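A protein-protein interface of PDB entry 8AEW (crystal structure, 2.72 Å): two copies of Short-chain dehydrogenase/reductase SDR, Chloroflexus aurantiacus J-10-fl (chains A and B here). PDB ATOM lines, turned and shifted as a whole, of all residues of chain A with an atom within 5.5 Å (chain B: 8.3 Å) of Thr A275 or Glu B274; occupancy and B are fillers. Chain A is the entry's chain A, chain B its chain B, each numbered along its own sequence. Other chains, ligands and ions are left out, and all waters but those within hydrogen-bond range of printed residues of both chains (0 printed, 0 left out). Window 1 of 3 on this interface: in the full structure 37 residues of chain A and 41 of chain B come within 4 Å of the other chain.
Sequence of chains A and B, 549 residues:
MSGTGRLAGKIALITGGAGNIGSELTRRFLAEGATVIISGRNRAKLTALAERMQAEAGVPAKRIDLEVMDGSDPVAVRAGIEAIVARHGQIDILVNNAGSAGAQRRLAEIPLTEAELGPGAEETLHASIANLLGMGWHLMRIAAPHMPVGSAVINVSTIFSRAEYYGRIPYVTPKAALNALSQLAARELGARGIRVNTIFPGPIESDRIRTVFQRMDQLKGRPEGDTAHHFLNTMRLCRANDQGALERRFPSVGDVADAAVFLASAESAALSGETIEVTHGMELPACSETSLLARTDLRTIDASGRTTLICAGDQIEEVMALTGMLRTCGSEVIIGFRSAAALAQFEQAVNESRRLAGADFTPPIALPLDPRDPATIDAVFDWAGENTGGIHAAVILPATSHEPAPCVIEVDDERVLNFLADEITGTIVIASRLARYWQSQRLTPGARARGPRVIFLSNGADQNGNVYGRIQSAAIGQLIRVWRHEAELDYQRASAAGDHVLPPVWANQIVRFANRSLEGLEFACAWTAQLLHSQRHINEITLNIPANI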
ATOM      1  N   GLN A 183      28.812 -28.684  21.739  1.00  0.00           N
ATOM      2  CA  GLN A 183      27.586 -29.394  21.365  1.00  0.00           C
ATOM      3  C   GLN A 183      27.805 -30.905  21.293  1.00  0.00           C
ATOM      4  O   GLN A 183      26.995 -31.694  21.787  1.00  0.00           O
ATOM      5  CB  GLN A 183      27.070 -28.869  20.036  1.00  0.00           C
ATOM      6  CG  GLN A 183      26.753 -27.387  20.049  1.00  0.00           C
ATOM      7  CD  GLN A 183      25.627 -27.031  21.002  1.00  0.00           C
ATOM      8  OE1 GLN A 183      24.703 -27.825  21.207  1.00  0.00           O
ATOM      9  NE2 GLN A 183      25.678 -25.811  21.562  1.00  0.00           N
ATOM     10  N   ASN A 197      27.290 -26.523  28.611  1.00  0.00           N
ATOM     11  CA  ASN A 197      26.598 -25.302  28.183  1.00  0.00           C
ATOM     12  C   ASN A 197      27.631 -24.206  27.927  1.00  0.00           C
ATOM     13  O   ASN A 197      28.778 -24.312  28.378  1.00  0.00           O
ATOM     14  CB  ASN A 197      25.573 -24.831  29.224  1.00  0.00           C
ATOM     15  CG  ASN A 197      24.363 -25.748  29.313  1.00  0.00           C
ATOM     16  OD1 ASN A 197      23.786 -26.112  28.302  1.00  0.00           O
ATOM     17  ND2 ASN A 197      24.004 -26.156  30.527  1.00  0.00           N
ATOM     18  N   THR A 198      27.227 -23.142  27.191  1.00  0.00           N
ATOM     19  CA  THR A 198      28.177 -22.168  26.644  1.00  0.00           C
ATOM     20  C   THR A 198      27.730 -20.712  26.856  1.00  0.00           C
ATOM     21  O   THR A 198      26.555 -20.380  26.688  1.00  0.00           O
ATOM     22  CB  THR A 198      28.427 -22.452  25.133  1.00  0.00           C
ATOM     23  OG1 THR A 198      28.820 -23.822  24.949  1.00  0.00           O
ATOM     24  CG2 THR A 198      29.564 -21.625  24.631  1.00  0.00           C
ATOM     25  N   ILE A 199      28.684 -19.842  27.223  1.00  0.00           N
ATOM     26  CA  ILE A 199      28.473 -18.401  27.424  1.00  0.00           C
ATOM     27  C   ILE A 199      29.249 -17.632  26.346  1.00  0.00           C
ATOM     28  O   ILE A 199      30.426 -17.918  26.104  1.00  0.00           O
ATOM     29  CB  ILE A 199      28.909 -17.966  28.846  1.00  0.00           C
ATOM     30  CG1 ILE A 199      28.175 -18.781  29.891  1.00  0.00           C
ATOM     31  CG2 ILE A 199      28.601 -16.507  29.159  1.00  0.00           C
ATOM     32  CD1 ILE A 199      28.826 -18.716  31.228  1.00  0.00           C
ATOM     33  N   PHE A 200      28.580 -16.680  25.678  1.00  0.00           N
ATOM     34  CA  PHE A 200      29.193 -15.795  24.686  1.00  0.00           C
ATOM     35  C   PHE A 200      29.239 -14.369  25.205  1.00  0.00           C
ATOM     36  O   PHE A 200      28.406 -13.534  24.816  1.00  0.00           O
ATOM     37  CB  PHE A 200      28.459 -15.790  23.339  1.00  0.00           C
ATOM     38  CG  PHE A 200      28.583 -17.042  22.530  1.00  0.00           C
ATOM     39  CD1 PHE A 200      28.979 -18.234  23.080  1.00  0.00           C
ATOM     40  CD2 PHE A 200      28.449 -16.965  21.165  1.00  0.00           C
ATOM     41  CE1 PHE A 200      29.113 -19.354  22.303  1.00  0.00           C
ATOM     42  CE2 PHE A 200      28.606 -18.077  20.398  1.00  0.00           C
ATOM     43  CZ  PHE A 200      28.943 -19.281  20.975  1.00  0.00           C
ATOM     44  N   ARG A 236      20.661  -4.226  20.692  1.00  0.00           N
ATOM     45  CA  ARG A 236      19.252  -3.915  20.839  1.00  0.00           C
ATOM     46  C   ARG A 236      18.911  -3.288  22.189  1.00  0.00           C
ATOM     47  O   ARG A 236      18.022  -2.430  22.239  1.00  0.00           O
ATOM     48  CB  ARG A 236      18.443  -5.193  20.599  1.00  0.00           C
ATOM     49  CG  ARG A 236      18.578  -5.654  19.154  1.00  0.00           C
ATOM     50  CD  ARG A 236      17.874  -6.936  18.837  1.00  0.00           C
ATOM     51  NE  ARG A 236      18.480  -8.103  19.460  1.00  0.00           N
ATOM     52  CZ  ARG A 236      18.062  -9.340  19.246  1.00  0.00           C
ATOM     53  NH1 ARG A 236      17.100  -9.602  18.367  1.00  0.00           N
ATOM     54  NH2 ARG A 236      18.655 -10.344  19.884  1.00  0.00           N
ATOM     55  N   GLY A 273      23.499 -28.135  26.041  1.00  0.00           N
ATOM     56  CA  GLY A 273      23.641 -27.650  24.688  1.00  0.00           C
ATOM     57  C   GLY A 273      23.086 -26.268  24.463  1.00  0.00           C
ATOM     58  O   GLY A 273      22.986 -25.839  23.305  1.00  0.00           O
ATOM     59  N   GLU A 274      22.713 -25.561  25.525  1.00  0.00           N
ATOM     60  CA  GLU A 274      22.210 -24.207  25.379  1.00  0.00           C
ATOM     61  C   GLU A 274      23.372 -23.210  25.265  1.00  0.00           C
ATOM     62  O   GLU A 274      24.532 -23.530  25.556  1.00  0.00           O
ATOM     63  CB  GLU A 274      21.275 -23.878  26.552  1.00  0.00           C
ATOM     64  CG  GLU A 274      20.564 -22.528  26.477  1.00  0.00           C
ATOM     65  CD  GLU A 274      19.686 -22.404  25.248  1.00  0.00           C
ATOM     66  OE1 GLU A 274      19.104 -23.443  24.825  1.00  0.00           O
ATOM     67  OE2 GLU A 274      19.640 -21.278  24.679  1.00  0.00           O
ATOM     68  N   THR A 275      23.061 -22.006  24.763  1.00  0.00           N
ATOM     69  CA  THR A 275      23.989 -20.881  24.741  1.00  0.00           C
ATOM     70  C   THR A 275      23.251 -19.632  25.227  1.00  0.00           C
ATOM     71  O   THR A 275      22.035 -19.500  25.042  1.00  0.00           O
ATOM     72  CB  THR A 275      24.621 -20.648  23.302  1.00  0.00           C
ATOM     73  OG1 THR A 275      25.266 -21.841  22.819  1.00  0.00           O
ATOM     74  CG2 THR A 275      25.687 -19.513  23.312  1.00  0.00           C
ATOM     75  N   ILE A 276      23.986 -18.746  25.899  1.00  0.00           N
ATOM     76  CA  ILE A 276      23.483 -17.496  26.472  1.00  0.00           C
ATOM     77  C   ILE A 276      24.450 -16.408  26.037  1.00  0.00           C
ATOM     78  O   ILE A 276      25.646 -16.461  26.380  1.00  0.00           O
ATOM     79  CB  ILE A 276      23.402 -17.553  28.016  1.00  0.00           C
ATOM     80  CG1 ILE A 276      22.452 -18.657  28.475  1.00  0.00           C
ATOM     81  CG2 ILE A 276      23.007 -16.197  28.634  1.00  0.00           C
ATOM     82  CD1 ILE A 276      22.548 -18.984  29.935  1.00  0.00           C
ATOM     83  N   GLU A 277      23.947 -15.409  25.313  1.00  0.00           N
ATOM     84  CA  GLU A 277      24.809 -14.370  24.754  1.00  0.00           C
ATOM     85  C   GLU A 277      24.718 -13.149  25.651  1.00  0.00           C
ATOM     86  O   GLU A 277      23.687 -12.471  25.685  1.00  0.00           O
ATOM     87  CB  GLU A 277      24.413 -14.033  23.316  1.00  0.00           C
ATOM     88  CG  GLU A 277      24.514 -15.209  22.378  1.00  0.00           C
ATOM     89  CD  GLU A 277      24.038 -14.900  20.961  1.00  0.00           C
ATOM     90  OE1 GLU A 277      23.654 -13.732  20.666  1.00  0.00           O
ATOM     91  OE2 GLU A 277      24.015 -15.865  20.157  1.00  0.00           O
ATOM     92  N   VAL B 153      10.124  -8.702  29.809  1.00  0.00           N
ATOM     93  CA  VAL B 153       9.047  -9.487  29.222  1.00  0.00           C
ATOM     94  C   VAL B 153       9.553 -10.910  29.038  1.00  0.00           C
ATOM     95  O   VAL B 153      10.617 -11.111  28.446  1.00  0.00           O
ATOM     96  CB  VAL B 153       8.586  -8.896  27.874  1.00  0.00           C
ATOM     97  CG1 VAL B 153       7.554  -9.799  27.229  1.00  0.00           C
ATOM     98  CG2 VAL B 153       8.005  -7.506  28.038  1.00  0.00           C
ATOM     99  N   ASN B 155       8.216 -14.296  27.141  1.00  0.00           N
ATOM    100  CA  ASN B 155       7.243 -14.954  26.277  1.00  0.00           C
ATOM    101  C   ASN B 155       7.487 -16.461  26.337  1.00  0.00           C
ATOM    102  O   ASN B 155       8.568 -16.939  25.979  1.00  0.00           O
ATOM    103  CB  ASN B 155       7.347 -14.420  24.843  1.00  0.00           C
ATOM    104  CG  ASN B 155       6.692 -13.005  24.656  1.00  0.00           C
ATOM    105  OD1 ASN B 155       5.548 -12.756  25.055  1.00  0.00           O
ATOM    106  ND2 ASN B 155       7.437 -12.090  24.046  1.00  0.00           N
ATOM    107  N   SER B 182       8.565 -11.895  19.132  1.00  0.00           N
ATOM    108  CA  SER B 182       9.419 -11.587  20.271  1.00  0.00           C
ATOM    109  C   SER B 182      10.728 -10.960  19.818  1.00  0.00           C
ATOM    110  O   SER B 182      11.083  -9.858  20.264  1.00  0.00           O
ATOM    111  CB  SER B 182       9.677 -12.848  21.088  1.00  0.00           C
ATOM    112  OG  SER B 182       8.498 -13.262  21.753  1.00  0.00           O
ATOM    113  N   GLN B 183      11.432 -11.622  18.893  1.00  0.00           N
ATOM    114  CA  GLN B 183      12.722 -11.128  18.418  1.00  0.00           C
ATOM    115  C   GLN B 183      12.647  -9.690  17.935  1.00  0.00           C
ATOM    116  O   GLN B 183      13.510  -8.861  18.252  1.00  0.00           O
ATOM    117  CB  GLN B 183      13.208 -12.007  17.284  1.00  0.00           C
ATOM    118  CG  GLN B 183      13.504 -13.383  17.727  1.00  0.00           C
ATOM    119  CD  GLN B 183      14.621 -13.385  18.751  1.00  0.00           C
ATOM    120  OE1 GLN B 183      15.534 -12.530  18.703  1.00  0.00           O
ATOM    121  NE2 GLN B 183      14.576 -14.358  19.679  1.00  0.00           N
ATOM    122  N   ALA B 186      12.203  -7.091  20.643  1.00  0.00           N
ATOM    123  CA  ALA B 186      13.408  -6.857  21.414  1.00  0.00           C
ATOM    124  C   ALA B 186      14.144  -5.615  20.909  1.00  0.00           C
ATOM    125  O   ALA B 186      14.641  -4.814  21.713  1.00  0.00           O
ATOM    126  CB  ALA B 186      14.289  -8.102  21.369  1.00  0.00           C
ATOM    127  N   ARG B 195      13.746  -5.641  28.439  1.00  0.00           N
ATOM    128  CA  ARG B 195      14.199  -6.928  27.953  1.00  0.00           C
ATOM    129  C   ARG B 195      13.007  -7.755  27.498  1.00  0.00           C
ATOM    130  O   ARG B 195      11.916  -7.663  28.077  1.00  0.00           O
ATOM    131  CB  ARG B 195      14.906  -7.702  29.063  1.00  0.00           C
ATOM    132  CG  ARG B 195      16.261  -7.178  29.545  1.00  0.00           C
ATOM    133  CD  ARG B 195      16.738  -8.071  30.695  1.00  0.00           C
ATOM    134  NE  ARG B 195      15.990  -7.763  31.910  1.00  0.00           N
ATOM    135  CZ  ARG B 195      15.864  -8.580  32.946  1.00  0.00           C
ATOM    136  NH1 ARG B 195      16.375  -9.806  32.924  1.00  0.00           N
ATOM    137  NH2 ARG B 195      15.225  -8.152  34.034  1.00  0.00           N
ATOM    138  N   VAL B 196      13.202  -8.536  26.432  1.00  0.00           N
ATOM    139  CA  VAL B 196      12.245  -9.559  26.018  1.00  0.00           C
ATOM    140  C   VAL B 196      13.062 -10.821  25.825  1.00  0.00           C
ATOM    141  O   VAL B 196      14.139 -10.756  25.234  1.00  0.00           O
ATOM    142  CB  VAL B 196      11.488  -9.183  24.723  1.00  0.00           C
ATOM    143  CG1 VAL B 196      10.378 -10.190  24.447  1.00  0.00           C
ATOM    144  CG2 VAL B 196      10.935  -7.763  24.782  1.00  0.00           C
ATOM    145  N   ASN B 197      12.592 -11.952  26.338  1.00  0.00           N
ATOM    146  CA  ASN B 197      13.360 -13.190  26.252  1.00  0.00           C
ATOM    147  C   ASN B 197      12.354 -14.327  26.288  1.00  0.00           C
ATOM    148  O   ASN B 197      11.211 -14.132  26.692  1.00  0.00           O
ATOM    149  CB  ASN B 197      14.389 -13.329  27.394  1.00  0.00           C
ATOM    150  CG  ASN B 197      15.587 -12.358  27.278  1.00  0.00           C
ATOM    151  OD1 ASN B 197      16.309 -12.344  26.280  1.00  0.00           O
ATOM    152  ND2 ASN B 197      15.768 -11.514  28.308  1.00  0.00           N
ATOM    153  N   THR B 198      12.773 -15.526  25.867  1.00  0.00           N
ATOM    154  CA  THR B 198      11.814 -16.578  25.547  1.00  0.00           C
ATOM    155  C   THR B 198      12.212 -17.907  26.154  1.00  0.00           C
ATOM    156  O   THR B 198      13.364 -18.331  26.031  1.00  0.00           O
ATOM    157  CB  THR B 198      11.687 -16.797  24.015  1.00  0.00           C
ATOM    158  OG1 THR B 198      11.467 -15.543  23.350  1.00  0.00           O
ATOM    159  CG2 THR B 198      10.553 -17.746  23.732  1.00  0.00           C
ATOM    160  N   ILE B 199      11.214 -18.604  26.700  1.00  0.00           N
ATOM    161  CA  ILE B 199      11.365 -19.939  27.277  1.00  0.00           C
ATOM    162  C   ILE B 199      10.640 -20.939  26.376  1.00  0.00           C
ATOM    163  O   ILE B 199       9.451 -20.768  26.088  1.00  0.00           O
ATOM    164  CB  ILE B 199      10.790 -19.989  28.707  1.00  0.00           C
ATOM    165  CG1 ILE B 199      11.423 -18.912  29.554  1.00  0.00           C
ATOM    166  CG2 ILE B 199      10.980 -21.374  29.356  1.00  0.00           C
ATOM    167  CD1 ILE B 199      10.823 -18.820  30.916  1.00  0.00           C
ATOM    168  N   PHE B 200      11.341 -22.004  25.981  1.00  0.00           N
ATOM    169  CA  PHE B 200      10.798 -23.107  25.189  1.00  0.00           C
ATOM    170  C   PHE B 200      10.719 -24.351  26.056  1.00  0.00           C
ATOM    171  O   PHE B 200      11.659 -25.158  26.068  1.00  0.00           O
ATOM    172  CB  PHE B 200      11.649 -23.424  23.947  1.00  0.00           C
ATOM    173  CG  PHE B 200      11.445 -22.512  22.760  1.00  0.00           C
ATOM    174  CD1 PHE B 200      10.522 -21.480  22.768  1.00  0.00           C
ATOM    175  CD2 PHE B 200      12.136 -22.762  21.584  1.00  0.00           C
ATOM    176  CE1 PHE B 200      10.353 -20.665  21.648  1.00  0.00           C
ATOM    177  CE2 PHE B 200      11.972 -21.953  20.460  1.00  0.00           C
ATOM    178  CZ  PHE B 200      11.076 -20.906  20.498  1.00  0.00           C
ATOM    179  N   PHE B 262      15.165 -16.683  36.649  1.00  0.00           N
ATOM    180  CA  PHE B 262      16.382 -16.137  36.056  1.00  0.00           C
ATOM    181  C   PHE B 262      16.088 -14.974  35.114  1.00  0.00           C
ATOM    182  O   PHE B 262      16.710 -13.910  35.198  1.00  0.00           O
ATOM    183  CB  PHE B 262      17.139 -17.244  35.327  1.00  0.00           C
ATOM    184  CG  PHE B 262      18.390 -16.766  34.652  1.00  0.00           C
ATOM    185  CD1 PHE B 262      19.471 -16.291  35.412  1.00  0.00           C
ATOM    186  CD2 PHE B 262      18.507 -16.810  33.269  1.00  0.00           C
ATOM    187  CE1 PHE B 262      20.633 -15.839  34.808  1.00  0.00           C
ATOM    188  CE2 PHE B 262      19.670 -16.360  32.643  1.00  0.00           C
ATOM    189  CZ  PHE B 262      20.737 -15.872  33.420  1.00  0.00           C
ATOM    190  N   LEU B 263      15.130 -15.160  34.204  1.00  0.00           N
ATOM    191  CA  LEU B 263      14.830 -14.131  33.215  1.00  0.00           C
ATOM    192  C   LEU B 263      13.976 -12.987  33.754  1.00  0.00           C
ATOM    193  O   LEU B 263      13.891 -11.936  33.110  1.00  0.00           O
ATOM    194  CB  LEU B 263      14.182 -14.781  32.011  1.00  0.00           C
ATOM    195  CG  LEU B 263      15.136 -15.674  31.206  1.00  0.00           C
ATOM    196  CD1 LEU B 263      14.310 -16.403  30.108  1.00  0.00           C
ATOM    197  CD2 LEU B 263      16.284 -14.847  30.616  1.00  0.00           C
ATOM    198  N   SER B 268      19.787 -11.447  34.891  1.00  0.00           N
ATOM    199  CA  SER B 268      19.806 -11.517  33.437  1.00  0.00           C
ATOM    200  C   SER B 268      19.625 -10.130  32.826  1.00  0.00           C
ATOM    201  O   SER B 268      19.018  -9.958  31.767  1.00  0.00           O
ATOM    202  CB  SER B 268      18.740 -12.496  32.940  1.00  0.00           C
ATOM    203  OG  SER B 268      17.418 -12.082  33.272  1.00  0.00           O
ATOM    204  N   ALA B 270      21.565  -8.183  31.310  1.00  0.00           N
ATOM    205  CA  ALA B 270      22.285  -7.904  30.083  1.00  0.00           C
ATOM    206  C   ALA B 270      21.779  -8.737  28.914  1.00  0.00           C
ATOM    207  O   ALA B 270      22.471  -8.828  27.900  1.00  0.00           O
ATOM    208  CB  ALA B 270      23.781  -8.132  30.296  1.00  0.00           C
ATOM    209  N   LEU B 271      20.590  -9.340  29.031  1.00  0.00           N
ATOM    210  CA  LEU B 271      20.077 -10.285  28.044  1.00  0.00           C
ATOM    211  C   LEU B 271      18.818  -9.737  27.357  1.00  0.00           C
ATOM    212  O   LEU B 271      17.887  -9.297  28.038  1.00  0.00           O
ATOM    213  CB  LEU B 271      19.769 -11.632  28.709  1.00  0.00           C
ATOM    214  CG  LEU B 271      20.934 -12.263  29.459  1.00  0.00           C
ATOM    215  CD1 LEU B 271      20.613 -13.689  29.892  1.00  0.00           C
ATOM    216  CD2 LEU B 271      22.276 -12.171  28.723  1.00  0.00           C
ATOM    217  N   SER B 272      18.773  -9.788  26.015  1.00  0.00           N
ATOM    218  CA  SER B 272      17.566  -9.450  25.246  1.00  0.00           C
ATOM    219  C   SER B 272      17.631 -10.100  23.861  1.00  0.00           C
ATOM    220  O   SER B 272      18.619  -9.934  23.136  1.00  0.00           O
ATOM    221  CB  SER B 272      17.383  -7.930  25.106  1.00  0.00           C
ATOM    222  OG  SER B 272      16.230  -7.596  24.339  1.00  0.00           O
ATOM    223  N   GLY B 273      16.581 -10.816  23.493  1.00  0.00           N
ATOM    224  CA  GLY B 273      16.630 -11.621  22.305  1.00  0.00           C
ATOM    225  C   GLY B 273      17.156 -13.013  22.519  1.00  0.00           C
ATOM    226  O   GLY B 273      17.398 -13.732  21.542  1.00  0.00           O
ATOM    227  N   GLU B 274      17.363 -13.411  23.759  1.00  0.00           N
ATOM    228  CA  GLU B 274      17.806 -14.757  24.062  1.00  0.00           C
ATOM    229  C   GLU B 274      16.640 -15.729  24.107  1.00  0.00           C
ATOM    230  O   GLU B 274      15.481 -15.348  24.298  1.00  0.00           O
ATOM    231  CB  GLU B 274      18.549 -14.803  25.404  1.00  0.00           C
ATOM    232  CG  GLU B 274      19.963 -14.390  25.282  1.00  0.00           C
ATOM    233  CD  GLU B 274      20.702 -15.315  24.327  1.00  0.00           C
ATOM    234  OE1 GLU B 274      20.479 -16.561  24.342  1.00  0.00           O
ATOM    235  OE2 GLU B 274      21.448 -14.768  23.496  1.00  0.00           O
ATOM    236  N   THR B 275      16.973 -17.007  23.973  1.00  0.00           N
ATOM    237  CA  THR B 275      16.036 -18.091  24.198  1.00  0.00           C
ATOM    238  C   THR B 275      16.727 -19.156  25.039  1.00  0.00           C
ATOM    239  O   THR B 275      17.948 -19.341  24.941  1.00  0.00           O
ATOM    240  CB  THR B 275      15.509 -18.687  22.852  1.00  0.00           C
ATOM    241  OG1 THR B 275      16.631 -18.977  22.010  1.00  0.00           O
ATOM    242  CG2 THR B 275      14.556 -17.726  22.140  1.00  0.00           C
ATOM    243  N   ILE B 276      15.932 -19.834  25.877  1.00  0.00           N
ATOM    244  CA  ILE B 276      16.374 -20.902  26.767  1.00  0.00           C
ATOM    245  C   ILE B 276      15.442 -22.082  26.555  1.00  0.00           C
ATOM    246  O   ILE B 276      14.222 -21.947  26.725  1.00  0.00           O
ATOM    247  CB  ILE B 276      16.353 -20.468  28.255  1.00  0.00           C
ATOM    248  CG1 ILE B 276      17.459 -19.453  28.561  1.00  0.00           C
ATOM    249  CG2 ILE B 276      16.408 -21.691  29.229  1.00  0.00           C
ATOM    250  CD1 ILE B 276      17.306 -18.764  29.921  1.00  0.00           C
ATOM    251  N   GLU B 277      15.998 -23.233  26.194  1.00  0.00           N
ATOM    252  CA  GLU B 277      15.187 -24.418  25.931  1.00  0.00           C
ATOM    253  C   GLU B 277      15.246 -25.375  27.121  1.00  0.00           C
ATOM    254  O   GLU B 277      16.270 -26.029  27.349  1.00  0.00           O
ATOM    255  CB  GLU B 277      15.640 -25.115  24.654  1.00  0.00           C
ATOM    256  CG  GLU B 277      15.496 -24.295  23.408  1.00  0.00           C
ATOM    257  CD  GLU B 277      16.043 -25.032  22.214  1.00  0.00           C
ATOM    258  OE1 GLU B 277      16.438 -26.224  22.368  1.00  0.00           O
ATOM    259  OE2 GLU B 277      16.142 -24.398  21.141  1.00  0.00           O
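O of Ala B186 touches CB of Arg A236, 3.98 Å away.
Arg A236 touches Gly B273.
CA of Ile B276 touches OE2 of Glu A274, at 3.9 Å.
Ile A276 touches Leu B271.
Ile A276 touches Glu B274 (CA to OE1, 3.8 Å).
Glu A277 touches Leu B271 (O to CD2, 3.4 Å).
Of the 11 printed residues of chain A, 5 touch a printed residue of chain B.
Printed residues of chain A that touch a printed residue of chain B: Arg A236, Glu A274, Thr A275, Ile A276 and Glu A277.
Of the 22 printed residues of chain B, 9 touch a printed residue of chain A.
Printed residues of chain B that touch a printed residue of chain A: Gln B183, Ala B186, Leu B271, Ser B272, Gly B273, Glu B274, Thr B275, Ile B276 and Glu B277.
Hydrophobic or aromatic side chains of chain B that line the printed part of chain A: Leu B271.
Along chain B the printed residues that touch a printed residue of chain A span positions 183 to 277.
Among the printed residues, no Asp or Glu carboxylate lies within 4 Å of a Lys or Arg side-chain nitrogen of the other chain.
The side-chain amide nitrogen (ND2) of Asn B197 lies within hydrogen-bond range of the backbone carbonyl oxygen (O) of Leu B271 (3.1 Å).
The backbone NH (N) of Gly B273 lies within hydrogen-bond range of the side-chain amide oxygen (OD1) of Asn B197 (3.2 Å).
The backbone NH (N) of Glu B274 is in hydrogen-bond range of the side-chain amide oxygen (OD1) of Asn B197 (2.9 Å).
N of Thr B198 is in hydrogen-bond range of O of Glu B274 (3.1 Å).
The backbone NH (N) of Glu A274 is in hydrogen-bond range of the side-chain amide oxygen (OD1) of Asn A197, at 3.0 Å.
The backbone carbonyl oxygen (O) of Ile A276 sits at hydrogen-bond distance from the backbone NH (N) of Phe A200 (3.0 Å).
Ile A199 touches none of the printed residues of chain B.
Printed residues of chain B within 4 Å of Arg A236: Gln B183 (3.3 Å), Ala B186 (3.98 Å), Ser B272 (3.3 Å) and Gly B273 (3.4 Å).
Of the printed residues of chain B, Glu A277 touches Leu B271 (3.4 Å) and Glu B274 (3.1 Å).
Printed residues of chain A within 4 Å of Gly B273: Arg A236.
Glu B274 touches just these residues of chain A: Thr A275 (3.4 Å), Ile A276 (3.8 Å) and Glu A277 (3.1 Å).
The nearest residue of chain B that does not touch Thr A275 is Thr B275 (4.1 Å).
OE1 of Gln B183 lies within hydrogen-bond range of NH1 of Arg A236 (3.3 Å).
The guanidinium group of Arg A236 is in hydrogen-bond range of the backbone carbonyl oxygen of Ser B272, at 3.3 Å.
The side-chain carboxylate (OE2) of Glu B274 lies close to the backbone NH (N) of Glu A277 (3.2 Å).
The backbone carbonyl oxygen (O) of Thr B275 sits close to the side-chain carboxylate (OE2) of Glu A274 (2.6 Å).
The backbone NH of Glu B277 sits at hydrogen-bond distance from the side-chain carboxylate of Glu A274 (3.4 Å).
The side-chain carboxylate of Glu B274 sits close to the backbone carbonyl oxygen of Thr A275, at 3.4 Å.
Glu A274 touches Thr B275, and with the chains exchanged Thr A275 touches Glu B274.
Glu A274 touches Ile B276, and with the chains exchanged Ile A276 touches Glu B274.
Glu A274 touches Glu B277, and with the chains exchanged Glu A277 touches Glu B274.
Positions printed for both chains: 183, 197, 198, 199, 200, 273, 274, 275, 276 and 277.
Of the 12 pairs that touch across the chains among the printed residues, 6 have their exchanged pair printed and touching as well.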
